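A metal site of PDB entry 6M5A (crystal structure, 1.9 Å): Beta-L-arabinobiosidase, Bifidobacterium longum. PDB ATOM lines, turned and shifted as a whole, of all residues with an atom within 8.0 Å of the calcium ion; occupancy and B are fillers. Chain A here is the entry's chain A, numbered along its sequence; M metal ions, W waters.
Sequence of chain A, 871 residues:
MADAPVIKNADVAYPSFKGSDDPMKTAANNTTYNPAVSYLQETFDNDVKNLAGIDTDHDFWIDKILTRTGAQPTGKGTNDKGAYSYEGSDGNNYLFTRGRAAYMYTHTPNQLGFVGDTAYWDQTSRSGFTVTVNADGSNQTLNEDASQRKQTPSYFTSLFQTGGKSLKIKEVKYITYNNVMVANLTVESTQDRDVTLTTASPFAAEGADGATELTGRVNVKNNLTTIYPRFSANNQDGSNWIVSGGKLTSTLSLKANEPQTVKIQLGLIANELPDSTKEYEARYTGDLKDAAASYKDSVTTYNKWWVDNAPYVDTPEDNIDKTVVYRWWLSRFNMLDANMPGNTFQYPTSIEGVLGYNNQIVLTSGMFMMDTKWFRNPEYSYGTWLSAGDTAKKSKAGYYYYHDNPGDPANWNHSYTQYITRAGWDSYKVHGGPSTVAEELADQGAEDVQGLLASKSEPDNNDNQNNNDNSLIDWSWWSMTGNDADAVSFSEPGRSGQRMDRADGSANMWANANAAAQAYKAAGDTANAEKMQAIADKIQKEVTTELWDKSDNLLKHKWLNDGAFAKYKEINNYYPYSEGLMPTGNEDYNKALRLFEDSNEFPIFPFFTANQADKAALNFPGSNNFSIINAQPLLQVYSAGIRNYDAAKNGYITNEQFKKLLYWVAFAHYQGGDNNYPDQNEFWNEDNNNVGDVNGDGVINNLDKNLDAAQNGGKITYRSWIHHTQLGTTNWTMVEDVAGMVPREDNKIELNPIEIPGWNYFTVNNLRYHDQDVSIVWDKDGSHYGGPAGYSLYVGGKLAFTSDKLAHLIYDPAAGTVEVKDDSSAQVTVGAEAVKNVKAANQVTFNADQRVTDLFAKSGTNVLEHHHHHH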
ATOM      1  N   VAL A 691      24.548  16.285  32.087  1.00  0.00           N
ATOM      2  CA  VAL A 691      26.010  15.949  32.109  1.00  0.00           C
ATOM      3  C   VAL A 691      26.614  16.137  30.716  1.00  0.00           C
ATOM      4  O   VAL A 691      25.861  16.290  29.752  1.00  0.00           O
ATOM      5  CB  VAL A 691      26.273  14.513  32.596  1.00  0.00           C
ATOM      6  CG1 VAL A 691      25.653  14.249  33.961  1.00  0.00           C
ATOM      7  CG2 VAL A 691      25.806  13.466  31.604  1.00  0.00           C
ATOM      8  N   GLY A 692      27.946  16.050  30.618  1.00  0.00           N
ATOM      9  CA  GLY A 692      28.710  16.103  29.367  1.00  0.00           C
ATOM     10  C   GLY A 692      29.217  14.732  28.988  1.00  0.00           C
ATOM     11  O   GLY A 692      28.649  13.738  29.463  1.00  0.00           O
ATOM     12  N   ASP A 693      30.256  14.666  28.147  1.00  0.00           N
ATOM     13  CA  ASP A 693      30.794  13.392  27.621  1.00  0.00           C
ATOM     14  C   ASP A 693      31.570  12.721  28.749  1.00  0.00           C
ATOM     15  O   ASP A 693      32.815  12.756  28.739  1.00  0.00           O
ATOM     16  CB  ASP A 693      31.654  13.585  26.381  1.00  0.00           C
ATOM     17  CG  ASP A 693      32.256  12.280  25.887  1.00  0.00           C
ATOM     18  OD1 ASP A 693      31.763  11.219  26.330  1.00  0.00           O
ATOM     19  OD2 ASP A 693      33.223  12.323  25.092  1.00  0.00           O
ATOM     20  N   VAL A 694      30.849  12.120  29.684  1.00  0.00           N
ATOM     21  CA  VAL A 694      31.431  11.538  30.923  1.00  0.00           C
ATOM     22  C   VAL A 694      32.277  10.313  30.575  1.00  0.00           C
ATOM     23  O   VAL A 694      33.179   9.999  31.362  1.00  0.00           O
ATOM     24  CB  VAL A 694      30.318  11.176  31.930  1.00  0.00           C
ATOM     25  CG1 VAL A 694      30.880  10.533  33.183  1.00  0.00           C
ATOM     26  CG2 VAL A 694      29.483  12.395  32.286  1.00  0.00           C
ATOM     27  N   ASN A 695      31.991   9.592  29.471  1.00  0.00           N
ATOM     28  CA  ASN A 695      32.748   8.345  29.154  1.00  0.00           C
ATOM     29  C   ASN A 695      33.817   8.633  28.080  1.00  0.00           C
ATOM     30  O   ASN A 695      34.603   7.715  27.814  1.00  0.00           O
ATOM     31  CB  ASN A 695      31.870   7.158  28.764  1.00  0.00           C
ATOM     32  CG  ASN A 695      31.125   7.302  27.453  1.00  0.00           C
ATOM     33  OD1 ASN A 695      31.063   8.384  26.848  1.00  0.00           O
ATOM     34  ND2 ASN A 695      30.504   6.225  27.026  1.00  0.00           N
ATOM     35  N   GLY A 696      33.830   9.852  27.528  1.00  0.00           N
ATOM     36  CA  GLY A 696      34.865  10.344  26.602  1.00  0.00           C
ATOM     37  C   GLY A 696      34.824   9.628  25.262  1.00  0.00           C
ATOM     38  O   GLY A 696      35.905   9.235  24.770  1.00  0.00           O
ATOM     39  N   ASP A 697      33.625   9.439  24.694  1.00  0.00           N
ATOM     40  CA  ASP A 697      33.421   8.709  23.417  1.00  0.00           C
ATOM     41  C   ASP A 697      32.970   9.704  22.340  1.00  0.00           C
ATOM     42  O   ASP A 697      32.777   9.279  21.190  1.00  0.00           O
ATOM     43  CB  ASP A 697      32.486   7.510  23.612  1.00  0.00           C
ATOM     44  CG  ASP A 697      31.009   7.795  23.865  1.00  0.00           C
ATOM     45  OD1 ASP A 697      30.564   8.994  23.801  1.00  0.00           O
ATOM     46  OD2 ASP A 697      30.299   6.809  24.100  1.00  0.00           O
ATOM     47  N   GLY A 698      32.859  10.980  22.674  1.00  0.00           N
ATOM     48  CA  GLY A 698      32.634  12.052  21.686  1.00  0.00           C
ATOM     49  C   GLY A 698      31.238  12.616  21.767  1.00  0.00           C
ATOM     50  O   GLY A 698      31.054  13.728  21.262  1.00  0.00           O
ATOM     51  N   VAL A 699      30.310  11.889  22.394  1.00  0.00           N
ATOM     52  CA  VAL A 699      28.849  12.174  22.337  1.00  0.00           C
ATOM     53  C   VAL A 699      28.277  12.193  23.774  1.00  0.00           C
ATOM     54  O   VAL A 699      28.833  11.509  24.665  1.00  0.00           O
ATOM     55  CB  VAL A 699      28.139  11.156  21.417  1.00  0.00           C
ATOM     56  CG1 VAL A 699      26.651  11.450  21.245  1.00  0.00           C
ATOM     57  CG2 VAL A 699      28.821  11.072  20.056  1.00  0.00           C
ATOM     58  N   ILE A 700      27.247  13.009  23.972  1.00  0.00           N
ATOM     59  CA  ILE A 700      26.405  13.057  25.205  1.00  0.00           C
ATOM     60  C   ILE A 700      25.118  12.244  24.965  1.00  0.00           C
ATOM     61  O   ILE A 700      24.162  12.795  24.402  1.00  0.00           O
ATOM     62  CB  ILE A 700      26.095  14.514  25.614  1.00  0.00           C
ATOM     63  CG1 ILE A 700      27.374  15.318  25.847  1.00  0.00           C
ATOM     64  CG2 ILE A 700      25.187  14.535  26.844  1.00  0.00           C
ATOM     65  CD1 ILE A 700      27.150  16.761  26.218  1.00  0.00           C
ATOM     66  N   ASN A 701      25.097  10.980  25.417  1.00  0.00           N
ATOM     67  CA  ASN A 701      23.906  10.100  25.338  1.00  0.00           C
ATOM     68  C   ASN A 701      23.600   9.497  26.725  1.00  0.00           C
ATOM     69  O   ASN A 701      24.064  10.027  27.774  1.00  0.00           O
ATOM     70  CB  ASN A 701      24.071   9.085  24.199  1.00  0.00           C
ATOM     71  CG  ASN A 701      25.222   8.113  24.383  1.00  0.00           C
ATOM     72  OD1 ASN A 701      25.617   7.813  25.513  1.00  0.00           O
ATOM     73  ND2 ASN A 701      25.737   7.578  23.289  1.00  0.00           N
ATOM     74  N   ASN A 702      22.812   8.431  26.764  1.00  0.00           N
ATOM     75  CA  ASN A 702      22.323   7.859  28.036  1.00  0.00           C
ATOM     76  C   ASN A 702      23.505   7.236  28.794  1.00  0.00           C
ATOM     77  O   ASN A 702      23.487   7.280  30.047  1.00  0.00           O
ATOM     78  CB  ASN A 702      21.126   6.940  27.779  1.00  0.00           C
ATOM     79  CG  ASN A 702      19.818   7.705  27.623  1.00  0.00           C
ATOM     80  OD1 ASN A 702      19.694   8.850  28.056  1.00  0.00           O
ATOM     81  ND2 ASN A 702      18.821   7.063  27.051  1.00  0.00           N
ATOM     82  N   LEU A 703      24.503   6.682  28.100  1.00  0.00           N
ATOM     83  CA  LEU A 703      25.689   6.066  28.752  1.00  0.00           C
ATOM     84  C   LEU A 703      26.306   7.074  29.717  1.00  0.00           C
ATOM     85  O   LEU A 703      26.712   6.668  30.813  1.00  0.00           O
ATOM     86  CB  LEU A 703      26.746   5.670  27.714  1.00  0.00           C
ATOM     87  CG  LEU A 703      26.290   4.696  26.651  1.00  0.00           C
ATOM     88  CD1 LEU A 703      27.499   4.094  25.952  1.00  0.00           C
ATOM     89  CD2 LEU A 703      25.407   3.611  27.245  1.00  0.00           C
ATOM     90  N   ASP A 704      26.377   8.333  29.296  1.00  0.00           N
ATOM     91  CA  ASP A 704      26.956   9.427  30.110  1.00  0.00           C
ATOM     92  C   ASP A 704      26.127   9.621  31.372  1.00  0.00           C
ATOM     93  O   ASP A 704      26.720   9.592  32.463  1.00  0.00           O
ATOM     94  CB  ASP A 704      27.068  10.726  29.315  1.00  0.00           C
ATOM     95  CG  ASP A 704      28.065  10.577  28.174  1.00  0.00           C
ATOM     96  OD1 ASP A 704      29.198  10.135  28.470  1.00  0.00           O
ATOM     97  OD2 ASP A 704      27.664  10.805  27.015  1.00  0.00           O
ATOM     98  N   LYS A 705      24.835   9.842  31.202  1.00  0.00           N
ATOM     99  CA  LYS A 705      23.870  10.104  32.309  1.00  0.00           C
ATOM    100  C   LYS A 705      23.923   8.959  33.317  1.00  0.00           C
ATOM    101  O   LYS A 705      23.965   9.243  34.544  1.00  0.00           O
ATOM    102  CB  LYS A 705      22.473  10.281  31.731  1.00  0.00           C
ATOM    103  CG  LYS A 705      22.295  11.594  31.001  1.00  0.00           C
ATOM    104  CD  LYS A 705      21.196  11.526  30.019  1.00  0.00           C
ATOM    105  CE  LYS A 705      20.867  12.855  29.409  1.00  0.00           C
ATOM    106  NZ  LYS A 705      19.733  12.681  28.483  1.00  0.00           N
ATOM    107  N   LEU A 707      26.441   6.494  33.653  1.00  0.00           N
ATOM    108  CA  LEU A 707      27.777   6.356  34.291  1.00  0.00           C
ATOM    109  C   LEU A 707      27.922   7.411  35.389  1.00  0.00           C
ATOM    110  O   LEU A 707      28.371   7.041  36.487  1.00  0.00           O
ATOM    111  CB  LEU A 707      28.890   6.502  33.241  1.00  0.00           C
ATOM    112  CG  LEU A 707      30.318   6.330  33.792  1.00  0.00           C
ATOM    113  CD1 LEU A 707      30.462   5.063  34.628  1.00  0.00           C
ATOM    114  CD2 LEU A 707      31.345   6.301  32.653  1.00  0.00           C
HETATM  115 CA    CA M   1      29.734   9.885  25.884  1.00  0.00          CA
HETATM  116  O   HOH W   1      28.159   8.063  25.439  1.00  0.00           O
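The calcium ion is bound by O of Val 699, OD1 of Asn 695, OD1 of Asp 697, water W1, OD1 of Asp 693, OD2 of Asp 704 and OD1 of Asp 704.
The backbone NH (N) of Gly 696 sits close to the side-chain carboxylate (OD1) of Asp 693 (2.8 Å). OD2 of Asp 693 is in hydrogen-bond range of N of Gly 698, at 2.8 Å. The side-chain carboxylate (OD1) of Asp 704 lies close to the backbone NH (N) of Val 694 (2.9 Å). The side-chain carboxylate (OD2) of Asp 704 sits close to the backbone NH (N) of Asn 701, 3.0 Å away.
Water W1 lies within hydrogen-bond range of the side-chain amide oxygen (OD1) of Asn 701 (2.6 Å), the side-chain carboxylate (OD2) of Asp 697 (2.8 Å) and the side-chain amide nitrogen (ND2) of Asn 695 (3.4 Å).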
